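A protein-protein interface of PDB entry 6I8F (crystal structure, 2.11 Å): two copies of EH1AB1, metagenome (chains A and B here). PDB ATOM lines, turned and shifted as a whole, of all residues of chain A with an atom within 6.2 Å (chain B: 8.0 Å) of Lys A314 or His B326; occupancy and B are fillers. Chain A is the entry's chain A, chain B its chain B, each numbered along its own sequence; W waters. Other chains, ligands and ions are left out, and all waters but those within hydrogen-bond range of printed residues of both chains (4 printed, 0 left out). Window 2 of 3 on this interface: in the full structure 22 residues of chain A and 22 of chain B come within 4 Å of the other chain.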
ATOM      1  N   ARG A 119       3.032  -4.939 -30.442  1.00  0.00           N
ATOM      2  CA  ARG A 119       2.602  -4.226 -29.245  1.00  0.00           C
ATOM      3  C   ARG A 119       1.603  -5.099 -28.485  1.00  0.00           C
ATOM      4  O   ARG A 119       1.681  -5.187 -27.266  1.00  0.00           O
ATOM      5  CB  ARG A 119       2.021  -2.851 -29.575  1.00  0.00           C
ATOM      6  CG  ARG A 119       1.805  -1.970 -28.356  1.00  0.00           C
ATOM      7  CD  ARG A 119       1.396  -0.543 -28.697  1.00  0.00           C
ATOM      8  NE  ARG A 119       1.189   0.241 -27.489  1.00  0.00           N
ATOM      9  CZ  ARG A 119       2.077   1.084 -26.960  1.00  0.00           C
ATOM     10  NH1 ARG A 119       3.204   1.330 -27.600  1.00  0.00           N
ATOM     11  NH2 ARG A 119       1.812   1.704 -25.813  1.00  0.00           N
ATOM     12  N   TYR A 295     -14.407   4.166 -28.069  1.00  0.00           N
ATOM     13  CA  TYR A 295     -13.385   5.220 -28.107  1.00  0.00           C
ATOM     14  C   TYR A 295     -13.984   6.427 -28.832  1.00  0.00           C
ATOM     15  O   TYR A 295     -13.977   6.472 -30.058  1.00  0.00           O
ATOM     16  CB  TYR A 295     -12.089   4.729 -28.769  1.00  0.00           C
ATOM     17  CG  TYR A 295     -11.148   4.022 -27.823  1.00  0.00           C
ATOM     18  CD1 TYR A 295     -11.497   2.814 -27.239  1.00  0.00           C
ATOM     19  CD2 TYR A 295      -9.921   4.570 -27.472  1.00  0.00           C
ATOM     20  CE1 TYR A 295     -10.659   2.171 -26.337  1.00  0.00           C
ATOM     21  CE2 TYR A 295      -9.068   3.935 -26.578  1.00  0.00           C
ATOM     22  CZ  TYR A 295      -9.443   2.729 -26.006  1.00  0.00           C
ATOM     23  OH  TYR A 295      -8.638   2.097 -25.108  1.00  0.00           O
ATOM     24  N   LEU A 309      -2.368   8.476 -34.566  1.00  0.00           N
ATOM     25  CA  LEU A 309      -3.414   8.491 -33.538  1.00  0.00           C
ATOM     26  C   LEU A 309      -2.930   7.731 -32.293  1.00  0.00           C
ATOM     27  O   LEU A 309      -2.906   6.494 -32.251  1.00  0.00           O
ATOM     28  CB  LEU A 309      -4.710   7.894 -34.103  1.00  0.00           C
ATOM     29  CG  LEU A 309      -5.258   8.551 -35.373  1.00  0.00           C
ATOM     30  CD1 LEU A 309      -6.523   7.859 -35.853  1.00  0.00           C
ATOM     31  CD2 LEU A 309      -5.517  10.037 -35.161  1.00  0.00           C
ATOM     32  N   SER A 310      -2.567   8.504 -31.265  1.00  0.00           N
ATOM     33  CA  SER A 310      -2.210   7.998 -29.947  1.00  0.00           C
ATOM     34  C   SER A 310      -3.321   7.134 -29.345  1.00  0.00           C
ATOM     35  O   SER A 310      -3.027   6.239 -28.556  1.00  0.00           O
ATOM     36  CB  SER A 310      -1.919   9.139 -29.019  1.00  0.00           C
ATOM     37  OG  SER A 310      -0.670   9.691 -29.363  1.00  0.00           O
ATOM     38  N   GLN A 311      -4.584   7.469 -29.648  1.00  0.00           N
ATOM     39  CA  GLN A 311      -5.718   6.733 -29.111  1.00  0.00           C
ATOM     40  C   GLN A 311      -5.562   5.262 -29.523  1.00  0.00           C
ATOM     41  O   GLN A 311      -5.944   4.350 -28.790  1.00  0.00           O
ATOM     42  CB  GLN A 311      -7.040   7.327 -29.608  1.00  0.00           C
ATOM     43  CG  GLN A 311      -7.469   8.593 -28.882  1.00  0.00           C
ATOM     44  CD  GLN A 311      -7.808   8.334 -27.435  1.00  0.00           C
ATOM     45  OE1 GLN A 311      -8.745   7.610 -27.111  1.00  0.00           O
ATOM     46  NE2 GLN A 311      -7.017   8.901 -26.545  1.00  0.00           N
ATOM     47  N   GLY A 312      -4.966   5.053 -30.705  1.00  0.00           N
ATOM     48  CA  GLY A 312      -4.710   3.731 -31.232  1.00  0.00           C
ATOM     49  C   GLY A 312      -3.805   2.916 -30.320  1.00  0.00           C
ATOM     50  O   GLY A 312      -4.023   1.721 -30.129  1.00  0.00           O
ATOM     51  N   LEU A 313      -2.784   3.558 -29.745  1.00  0.00           N
ATOM     52  CA  LEU A 313      -1.873   2.858 -28.837  1.00  0.00           C
ATOM     53  C   LEU A 313      -2.582   2.548 -27.509  1.00  0.00           C
ATOM     54  O   LEU A 313      -2.374   1.485 -26.934  1.00  0.00           O
ATOM     55  CB  LEU A 313      -0.621   3.704 -28.605  1.00  0.00           C
ATOM     56  CG  LEU A 313       0.240   3.946 -29.842  1.00  0.00           C
ATOM     57  CD1 LEU A 313       1.384   4.890 -29.503  1.00  0.00           C
ATOM     58  CD2 LEU A 313       0.781   2.640 -30.419  1.00  0.00           C
ATOM     59  N   LYS A 314      -3.402   3.487 -27.029  1.00  0.00           N
ATOM     60  CA  LYS A 314      -4.216   3.260 -25.840  1.00  0.00           C
ATOM     61  C   LYS A 314      -5.148   2.063 -26.074  1.00  0.00           C
ATOM     62  O   LYS A 314      -5.246   1.217 -25.202  1.00  0.00           O
ATOM     63  CB  LYS A 314      -4.996   4.524 -25.472  1.00  0.00           C
ATOM     64  CG  LYS A 314      -4.127   5.706 -25.066  1.00  0.00           C
ATOM     65  CD  LYS A 314      -4.151   6.013 -23.584  1.00  0.00           C
ATOM     66  CE  LYS A 314      -2.884   6.691 -23.097  1.00  0.00           C
ATOM     67  NZ  LYS A 314      -2.637   7.953 -23.840  1.00  0.00           N
ATOM     68  N   ALA A 315      -5.779   1.990 -27.265  1.00  0.00           N
ATOM     69  CA  ALA A 315      -6.695   0.906 -27.629  1.00  0.00           C
ATOM     70  C   ALA A 315      -5.954  -0.435 -27.716  1.00  0.00           C
ATOM     71  O   ALA A 315      -6.482  -1.458 -27.238  1.00  0.00           O
ATOM     72  CB  ALA A 315      -7.403   1.202 -28.920  1.00  0.00           C
ATOM     73  N   ASN A 316      -4.774  -0.424 -28.350  1.00  0.00           N
ATOM     74  CA  ASN A 316      -3.854  -1.574 -28.383  1.00  0.00           C
ATOM     75  C   ASN A 316      -3.661  -2.099 -26.955  1.00  0.00           C
ATOM     76  O   ASN A 316      -3.900  -3.279 -26.666  1.00  0.00           O
ATOM     77  CB  ASN A 316      -2.480  -1.232 -28.978  1.00  0.00           C
ATOM     78  CG  ASN A 316      -2.451  -0.938 -30.469  1.00  0.00           C
ATOM     79  OD1 ASN A 316      -1.419  -0.477 -30.978  1.00  0.00           O
ATOM     80  ND2 ASN A 316      -3.543  -1.194 -31.180  1.00  0.00           N
ATOM     81  N   ASP A 317      -3.225  -1.201 -26.065  1.00  0.00           N
ATOM     82  CA  ASP A 317      -2.878  -1.558 -24.685  1.00  0.00           C
ATOM     83  C   ASP A 317      -4.112  -2.094 -23.939  1.00  0.00           C
ATOM     84  O   ASP A 317      -4.001  -3.042 -23.157  1.00  0.00           O
ATOM     85  CB  ASP A 317      -2.228  -0.369 -23.972  1.00  0.00           C
ATOM     86  CG  ASP A 317      -0.893   0.022 -24.589  1.00  0.00           C
ATOM     87  OD1 ASP A 317      -0.410  -0.721 -25.484  1.00  0.00           O
ATOM     88  OD2 ASP A 317      -0.352   1.078 -24.206  1.00  0.00           O
ATOM     89  N   GLU A 318      -5.288  -1.485 -24.157  1.00  0.00           N
ATOM     90  CA  GLU A 318      -6.512  -1.943 -23.484  1.00  0.00           C
ATOM     91  C   GLU A 318      -6.913  -3.351 -23.966  1.00  0.00           C
ATOM     92  O   GLU A 318      -7.247  -4.217 -23.169  1.00  0.00           O
ATOM     93  CB  GLU A 318      -7.672  -0.967 -23.684  1.00  0.00           C
ATOM     94  CG  GLU A 318      -8.924  -1.440 -22.989  1.00  0.00           C
ATOM     95  CD  GLU A 318     -10.083  -0.465 -22.910  1.00  0.00           C
ATOM     96  OE1 GLU A 318      -9.997   0.647 -23.491  1.00  0.00           O
ATOM     97  OE2 GLU A 318     -11.077  -0.842 -22.281  1.00  0.00           O
ATOM     98  N   ALA A 319      -6.913  -3.571 -25.278  1.00  0.00           N
ATOM     99  CA  ALA A 319      -7.266  -4.879 -25.841  1.00  0.00           C
ATOM    100  C   ALA A 319      -6.324  -5.959 -25.281  1.00  0.00           C
ATOM    101  O   ALA A 319      -6.764  -7.006 -24.788  1.00  0.00           O
ATOM    102  CB  ALA A 319      -7.201  -4.814 -27.345  1.00  0.00           C
ATOM    103  N   PRO B  95       0.876   7.179 -11.228  1.00  0.00           N
ATOM    104  CA  PRO B  95      -0.572   7.199 -11.431  1.00  0.00           C
ATOM    105  C   PRO B  95      -1.166   6.471 -10.215  1.00  0.00           C
ATOM    106  O   PRO B  95      -0.576   5.515  -9.723  1.00  0.00           O
ATOM    107  CB  PRO B  95      -0.769   6.488 -12.773  1.00  0.00           C
ATOM    108  CG  PRO B  95       0.468   5.620 -12.911  1.00  0.00           C
ATOM    109  CD  PRO B  95       1.584   6.386 -12.241  1.00  0.00           C
ATOM    110  N   SER B 124      -1.920  -3.115 -12.074  1.00  0.00           N
ATOM    111  CA  SER B 124      -2.090  -1.854 -12.805  1.00  0.00           C
ATOM    112  C   SER B 124      -0.759  -1.107 -12.949  1.00  0.00           C
ATOM    113  O   SER B 124      -0.636  -0.251 -13.847  1.00  0.00           O
ATOM    114  CB  SER B 124      -3.113  -0.958 -12.138  1.00  0.00           C
ATOM    115  OG  SER B 124      -2.639  -0.483 -10.884  1.00  0.00           O
ATOM    116  N   CYS B 126       0.004   0.971 -10.734  1.00  0.00           N
ATOM    117  CA  CYS B 126      -0.415   2.222 -10.153  1.00  0.00           C
ATOM    118  C   CYS B 126      -0.379   2.084  -8.635  1.00  0.00           C
ATOM    119  O   CYS B 126      -0.622   1.014  -8.102  1.00  0.00           O
ATOM    120  CB  CYS B 126      -1.838   2.586 -10.559  1.00  0.00           C
ATOM    121  SG  CYS B 126      -2.086   2.739 -12.345  1.00  0.00           S
ATOM    122  N   ALA B 167      -1.885  14.377 -12.707  1.00  0.00           N
ATOM    123  CA  ALA B 167      -2.486  14.216 -14.025  1.00  0.00           C
ATOM    124  C   ALA B 167      -3.091  12.813 -14.201  1.00  0.00           C
ATOM    125  O   ALA B 167      -3.812  12.583 -15.158  1.00  0.00           O
ATOM    126  CB  ALA B 167      -1.449  14.476 -15.087  1.00  0.00           C
ATOM    127  N   ARG B 168      -2.790  11.867 -13.307  1.00  0.00           N
ATOM    128  CA  ARG B 168      -3.324  10.506 -13.455  1.00  0.00           C
ATOM    129  C   ARG B 168      -3.833   9.997 -12.100  1.00  0.00           C
ATOM    130  O   ARG B 168      -3.276   9.075 -11.496  1.00  0.00           O
ATOM    131  CB  ARG B 168      -2.267   9.586 -14.069  1.00  0.00           C
ATOM    132  CG  ARG B 168      -1.912   9.954 -15.503  1.00  0.00           C
ATOM    133  CD  ARG B 168      -0.839   9.042 -16.056  1.00  0.00           C
ATOM    134  NE  ARG B 168       0.434   9.221 -15.369  1.00  0.00           N
ATOM    135  CZ  ARG B 168       1.442   8.351 -15.409  1.00  0.00           C
ATOM    136  NH1 ARG B 168       1.291   7.209 -16.061  1.00  0.00           N
ATOM    137  NH2 ARG B 168       2.592   8.633 -14.804  1.00  0.00           N
ATOM    138  N   LEU B 169      -4.929  10.613 -11.663  1.00  0.00           N
ATOM    139  CA  LEU B 169      -5.559  10.340 -10.397  1.00  0.00           C
ATOM    140  C   LEU B 169      -6.912   9.694 -10.693  1.00  0.00           C
ATOM    141  O   LEU B 169      -7.769  10.339 -11.271  1.00  0.00           O
ATOM    142  CB  LEU B 169      -5.736  11.682  -9.683  1.00  0.00           C
ATOM    143  CG  LEU B 169      -5.096  11.852  -8.314  1.00  0.00           C
ATOM    144  CD1 LEU B 169      -3.630  11.429  -8.317  1.00  0.00           C
ATOM    145  CD2 LEU B 169      -5.227  13.305  -7.860  1.00  0.00           C
ATOM    146  N   ALA B 170      -7.077   8.419 -10.336  1.00  0.00           N
ATOM    147  CA  ALA B 170      -8.337   7.718 -10.531  1.00  0.00           C
ATOM    148  C   ALA B 170      -9.081   7.605  -9.195  1.00  0.00           C
ATOM    149  O   ALA B 170      -8.493   7.739  -8.130  1.00  0.00           O
ATOM    150  CB  ALA B 170      -8.076   6.366 -11.151  1.00  0.00           C
ATOM    151  N   PRO B 196     -11.411  13.445 -11.020  1.00  0.00           N
ATOM    152  CA  PRO B 196     -10.599  12.284 -11.369  1.00  0.00           C
ATOM    153  C   PRO B 196     -10.326  12.168 -12.876  1.00  0.00           C
ATOM    154  O   PRO B 196     -11.112  12.606 -13.681  1.00  0.00           O
ATOM    155  CB  PRO B 196     -11.468  11.106 -10.893  1.00  0.00           C
ATOM    156  CG  PRO B 196     -12.251  11.665  -9.734  1.00  0.00           C
ATOM    157  CD  PRO B 196     -12.540  13.092 -10.138  1.00  0.00           C
ATOM    158  N   ALA B 197      -9.195  11.564 -13.226  1.00  0.00           N
ATOM    159  CA  ALA B 197      -8.868  11.301 -14.601  1.00  0.00           C
ATOM    160  C   ALA B 197      -9.571  10.026 -15.068  1.00  0.00           C
ATOM    161  O   ALA B 197      -9.683   9.804 -16.268  1.00  0.00           O
ATOM    162  CB  ALA B 197      -7.375  11.174 -14.758  1.00  0.00           C
ATOM    163  N   PHE B 198     -10.044   9.201 -14.125  1.00  0.00           N
ATOM    164  CA  PHE B 198     -10.579   7.870 -14.452  1.00  0.00           C
ATOM    165  C   PHE B 198     -11.478   7.396 -13.316  1.00  0.00           C
ATOM    166  O   PHE B 198     -11.231   7.739 -12.155  1.00  0.00           O
ATOM    167  CB  PHE B 198      -9.427   6.890 -14.691  1.00  0.00           C
ATOM    168  CG  PHE B 198      -9.807   5.537 -15.232  1.00  0.00           C
ATOM    169  CD1 PHE B 198      -9.949   4.450 -14.387  1.00  0.00           C
ATOM    170  CD2 PHE B 198     -10.010   5.345 -16.589  1.00  0.00           C
ATOM    171  CE1 PHE B 198     -10.296   3.200 -14.882  1.00  0.00           C
ATOM    172  CE2 PHE B 198     -10.335   4.090 -17.089  1.00  0.00           C
ATOM    173  CZ  PHE B 198     -10.481   3.019 -16.236  1.00  0.00           C
ATOM    174  N   GLN B 199     -12.527   6.634 -13.649  1.00  0.00           N
ATOM    175  CA  GLN B 199     -13.414   6.067 -12.614  1.00  0.00           C
ATOM    176  C   GLN B 199     -13.560   4.550 -12.824  1.00  0.00           C
ATOM    177  O   GLN B 199     -13.918   4.071 -13.907  1.00  0.00           O
ATOM    178  CB  GLN B 199     -14.753   6.804 -12.555  1.00  0.00           C
ATOM    179  CG  GLN B 199     -15.567   6.762 -13.833  1.00  0.00           C
ATOM    180  CD  GLN B 199     -16.806   7.615 -13.733  1.00  0.00           C
ATOM    181  OE1 GLN B 199     -17.566   7.540 -12.756  1.00  0.00           O
ATOM    182  NE2 GLN B 199     -17.010   8.431 -14.755  1.00  0.00           N
ATOM    183  N   PRO B 260     -15.280  11.628 -16.190  1.00  0.00           N
ATOM    184  CA  PRO B 260     -14.066  11.009 -16.694  1.00  0.00           C
ATOM    185  C   PRO B 260     -14.257   9.623 -17.304  1.00  0.00           C
ATOM    186  O   PRO B 260     -15.208   8.916 -16.985  1.00  0.00           O
ATOM    187  CB  PRO B 260     -13.164  10.914 -15.460  1.00  0.00           C
ATOM    188  CG  PRO B 260     -14.099  10.925 -14.281  1.00  0.00           C
ATOM    189  CD  PRO B 260     -15.357  11.639 -14.721  1.00  0.00           C
ATOM    190  N   PRO B 261     -13.290   9.183 -18.140  1.00  0.00           N
ATOM    191  CA  PRO B 261     -13.253   7.813 -18.650  1.00  0.00           C
ATOM    192  C   PRO B 261     -13.511   6.782 -17.545  1.00  0.00           C
ATOM    193  O   PRO B 261     -13.062   6.964 -16.402  1.00  0.00           O
ATOM    194  CB  PRO B 261     -11.826   7.684 -19.196  1.00  0.00           C
ATOM    195  CG  PRO B 261     -11.457   9.097 -19.611  1.00  0.00           C
ATOM    196  CD  PRO B 261     -12.145   9.986 -18.597  1.00  0.00           C
ATOM    197  N   ALA B 262     -14.227   5.715 -17.907  1.00  0.00           N
ATOM    198  CA  ALA B 262     -14.772   4.786 -16.937  1.00  0.00           C
ATOM    199  C   ALA B 262     -14.499   3.322 -17.315  1.00  0.00           C
ATOM    200  O   ALA B 262     -14.484   2.924 -18.478  1.00  0.00           O
ATOM    201  CB  ALA B 262     -16.248   5.025 -16.822  1.00  0.00           C
ATOM    202  N   LYS B 289     -15.357   7.946 -22.942  1.00  0.00           N
ATOM    203  CA  LYS B 289     -14.636   6.681 -23.123  1.00  0.00           C
ATOM    204  C   LYS B 289     -15.008   5.754 -21.964  1.00  0.00           C
ATOM    205  O   LYS B 289     -14.665   6.033 -20.825  1.00  0.00           O
ATOM    206  CB  LYS B 289     -13.119   6.882 -23.180  1.00  0.00           C
ATOM    207  CG  LYS B 289     -12.325   5.592 -23.356  1.00  0.00           C
ATOM    208  CD  LYS B 289     -10.824   5.726 -23.217  1.00  0.00           C
ATOM    209  CE  LYS B 289     -10.174   6.371 -24.431  1.00  0.00           C
ATOM    210  NZ  LYS B 289      -8.740   6.708 -24.215  1.00  0.00           N
ATOM    211  N   THR B 291     -15.551   1.580 -20.702  1.00  0.00           N
ATOM    212  CA  THR B 291     -15.423   0.139 -20.789  1.00  0.00           C
ATOM    213  C   THR B 291     -16.445  -0.490 -19.838  1.00  0.00           C
ATOM    214  O   THR B 291     -16.426  -0.212 -18.631  1.00  0.00           O
ATOM    215  CB  THR B 291     -13.996  -0.318 -20.456  1.00  0.00           C
ATOM    216  OG1 THR B 291     -13.089   0.374 -21.317  1.00  0.00           O
ATOM    217  CG2 THR B 291     -13.789  -1.812 -20.607  1.00  0.00           C
ATOM    218  N   ALA B 319      -9.791  -5.040 -14.175  1.00  0.00           N
ATOM    219  CA  ALA B 319      -9.968  -3.659 -13.733  1.00  0.00           C
ATOM    220  C   ALA B 319      -8.599  -2.953 -13.705  1.00  0.00           C
ATOM    221  O   ALA B 319      -8.426  -1.878 -14.275  1.00  0.00           O
ATOM    222  CB  ALA B 319     -10.665  -3.642 -12.386  1.00  0.00           C
ATOM    223  N   ALA B 320      -7.614  -3.598 -13.062  1.00  0.00           N
ATOM    224  CA  ALA B 320      -6.260  -3.069 -12.950  1.00  0.00           C
ATOM    225  C   ALA B 320      -5.636  -2.857 -14.334  1.00  0.00           C
ATOM    226  O   ALA B 320      -5.001  -1.843 -14.559  1.00  0.00           O
ATOM    227  CB  ALA B 320      -5.405  -3.997 -12.121  1.00  0.00           C
ATOM    228  N   ALA B 321      -5.823  -3.812 -15.247  1.00  0.00           N
ATOM    229  CA  ALA B 321      -5.181  -3.759 -16.558  1.00  0.00           C
ATOM    230  C   ALA B 321      -5.776  -2.635 -17.417  1.00  0.00           C
ATOM    231  O   ALA B 321      -5.055  -1.915 -18.111  1.00  0.00           O
ATOM    232  CB  ALA B 321      -5.297  -5.091 -17.233  1.00  0.00           C
ATOM    233  N   VAL B 322      -7.098  -2.468 -17.362  1.00  0.00           N
ATOM    234  CA  VAL B 322      -7.750  -1.411 -18.130  1.00  0.00           C
ATOM    235  C   VAL B 322      -7.284  -0.040 -17.613  1.00  0.00           C
ATOM    236  O   VAL B 322      -6.965   0.863 -18.412  1.00  0.00           O
ATOM    237  CB  VAL B 322      -9.278  -1.550 -18.076  1.00  0.00           C
ATOM    238  CG1 VAL B 322      -9.981  -0.329 -18.638  1.00  0.00           C
ATOM    239  CG2 VAL B 322      -9.730  -2.807 -18.786  1.00  0.00           C
ATOM    240  N   MET B 323      -7.239   0.115 -16.283  1.00  0.00           N
ATOM    241  CA  MET B 323      -6.782   1.369 -15.677  1.00  0.00           C
ATOM    242  C   MET B 323      -5.328   1.661 -16.074  1.00  0.00           C
ATOM    243  O   MET B 323      -4.996   2.786 -16.462  1.00  0.00           O
ATOM    244  CB  MET B 323      -6.872   1.342 -14.153  1.00  0.00           C
ATOM    245  CG  MET B 323      -6.453   2.668 -13.534  1.00  0.00           C
ATOM    246  SD  MET B 323      -6.726   2.715 -11.751  1.00  0.00           S
ATOM    247  CE  MET B 323      -5.602   1.417 -11.249  1.00  0.00           C
ATOM    248  N   GLY B 324      -4.465   0.655 -15.922  1.00  0.00           N
ATOM    249  CA  GLY B 324      -3.069   0.743 -16.301  1.00  0.00           C
ATOM    250  C   GLY B 324      -2.904   1.114 -17.771  1.00  0.00           C
ATOM    251  O   GLY B 324      -2.084   1.976 -18.109  1.00  0.00           O
ATOM    252  N   ALA B 325      -3.668   0.456 -18.655  1.00  0.00           N
ATOM    253  CA  ALA B 325      -3.623   0.762 -20.075  1.00  0.00           C
ATOM    254  C   ALA B 325      -4.050   2.219 -20.310  1.00  0.00           C
ATOM    255  O   ALA B 325      -3.496   2.913 -21.169  1.00  0.00           O
ATOM    256  CB  ALA B 325      -4.487  -0.196 -20.851  1.00  0.00           C
ATOM    257  N   HIS B 326      -5.036   2.696 -19.548  1.00  0.00           N
ATOM    258  CA  HIS B 326      -5.495   4.064 -19.703  1.00  0.00           C
ATOM    259  C   HIS B 326      -4.378   5.055 -19.329  1.00  0.00           C
ATOM    260  O   HIS B 326      -4.216   6.078 -19.975  1.00  0.00           O
ATOM    261  CB  HIS B 326      -6.758   4.325 -18.883  1.00  0.00           C
ATOM    262  CG  HIS B 326      -7.310   5.685 -19.110  1.00  0.00           C
ATOM    263  ND1 HIS B 326      -7.968   6.024 -20.283  1.00  0.00           N
ATOM    264  CD2 HIS B 326      -7.274   6.801 -18.352  1.00  0.00           C
ATOM    265  CE1 HIS B 326      -8.345   7.288 -20.218  1.00  0.00           C
ATOM    266  NE2 HIS B 326      -7.912   7.795 -19.048  1.00  0.00           N
ATOM    267  N   PHE B 327      -3.629   4.736 -18.271  1.00  0.00           N
ATOM    268  CA  PHE B 327      -2.625   5.639 -17.691  1.00  0.00           C
ATOM    269  C   PHE B 327      -1.236   5.446 -18.321  1.00  0.00           C
ATOM    270  O   PHE B 327      -0.287   6.123 -17.939  1.00  0.00           O
ATOM    271  CB  PHE B 327      -2.588   5.443 -16.175  1.00  0.00           C
ATOM    272  CG  PHE B 327      -3.691   6.138 -15.416  1.00  0.00           C
ATOM    273  CD1 PHE B 327      -4.319   7.273 -15.920  1.00  0.00           C
ATOM    274  CD2 PHE B 327      -4.063   5.693 -14.159  1.00  0.00           C
ATOM    275  CE1 PHE B 327      -5.316   7.922 -15.199  1.00  0.00           C
ATOM    276  CE2 PHE B 327      -5.056   6.344 -13.437  1.00  0.00           C
ATOM    277  CZ  PHE B 327      -5.670   7.468 -13.949  1.00  0.00           C
ATOM    278  N   GLY B 328      -1.122   4.510 -19.266  1.00  0.00           N
ATOM    279  CA  GLY B 328       0.106   4.275 -19.999  1.00  0.00           C
ATOM    280  C   GLY B 328       1.198   3.640 -19.150  1.00  0.00           C
ATOM    281  O   GLY B 328       2.360   3.933 -19.367  1.00  0.00           O
ATOM    282  N   THR B 329       0.829   2.770 -18.202  1.00  0.00           N
ATOM    283  CA  THR B 329       1.801   2.135 -17.315  1.00  0.00           C
ATOM    284  C   THR B 329       2.379   0.901 -18.005  1.00  0.00           C
ATOM    285  O   THR B 329       1.906   0.485 -19.054  1.00  0.00           O
ATOM    286  CB  THR B 329       1.200   1.705 -15.967  1.00  0.00           C
ATOM    287  OG1 THR B 329       0.305   0.607 -16.169  1.00  0.00           O
ATOM    288  CG2 THR B 329       0.487   2.832 -15.255  1.00  0.00           C
ATOM    289  OXT THR B 329       3.312   0.307 -17.486  1.00  0.00           O
HETATM  290  O   HOH W   1       0.320   0.605 -20.936  1.00  0.00           O
HETATM  291  O   HOH W   2      -7.912   1.358 -20.895  1.00  0.00           O
HETATM  292  O   HOH W   3      -1.589   2.859 -22.959  1.00  0.00           O
HETATM  293  O   HOH W   4      -6.203   2.667 -22.807  1.00  0.00           O
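OE2 of Glu A318 sits at hydrogen-bond distance from OG1 of Thr B291 (2.5 Å). The side-chain amide oxygen (OE1) of Gln A311 is in hydrogen-bond range of the side-chain amino group (NZ) of Lys B289 (3.0 Å).
O of Ala B262 sits at hydrogen-bond distance from N of Thr B291 (2.8 Å). The side-chain hydroxyl (OH) of Tyr A295 lies within hydrogen-bond range of the side-chain carboxylate (OE1) of Glu A318. The guanidinium group (NE) of Arg A119 is in salt-bridge range of the side-chain carboxylate (OD1) of Asp A317, at 2.7 Å. O of Lys B289 sits at hydrogen-bond distance from N of Ala B262 (3.0 Å).
Among the printed residues, merely in contact across the chains: Tyr A295 with Lys B289 (3.4 Å), Lys A314 with Ala B325 (3.98 Å), Lys A314 with His B326 (3.4 Å), Asp A317 with Ala B325 (3.6 Å), Glu A318 with Val B322 (3.8 Å) and Glu A318 with Ala B325 (3.6 Å).
Of the printed residues of chain B, Tyr A295 touches Lys B289. No residue of chain B comes within 4 Å of Ala A315. Printed residues of chain A within 4 Å of Lys B289: Tyr A295 (3.4 Å) and Gln A311 (3.0 Å). Printed residues of chain A within 4 Å of Val B322: Glu A318 (3.8 Å). Of the printed residues of chain A, Ala B325 touches Lys A314 (3.98 Å), Asp A317 (3.6 Å) and Glu A318 (3.6 Å). His B326 touches just one residue of chain A: Lys A314 (3.4 Å). The nearest printed residue of chain B that does not touch Lys A314 is Lys B289 (4.5 Å).
Of the 13 printed residues of chain A, 5 touch a printed residue of chain B. Of the 27 printed residues of chain B, 5 touch a printed residue of chain A. Printed residues of chain B that touch a printed residue of chain A: Lys B289, Thr B291, Val B322, Ala B325 and His B326. Along chain B the printed residues that touch a printed residue of chain A span positions 289 to 326. Among the printed residues, 8 pairs touch across the chains.
1 position is printed for both chains. Of the 8 pairs that touch across the chains among the printed residues, none has its exchanged pair printed and touching as well.
Water W1 bridges the chain-end carboxylate of Thr B329 (2.5 Å) and the side-chain carboxylate of Asp A317 (3.4 Å). Water W3 lies within hydrogen-bond range of OD2 of Asp A317 (2.5 Å) and O of Ala B325 (2.6 Å). Water W2 lies within hydrogen-bond range of O of Val B322 (2.7 Å), OE1 of Glu A318 (3.4 Å) and N of His B326 (3.4 Å). Water W4 lies within hydrogen-bond range of O of Lys A314 (3.0 Å), O of Ala B325 (3.2 Å), OH of Tyr A295 (3.4 Å) and N of His B326 (3.5 Å).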
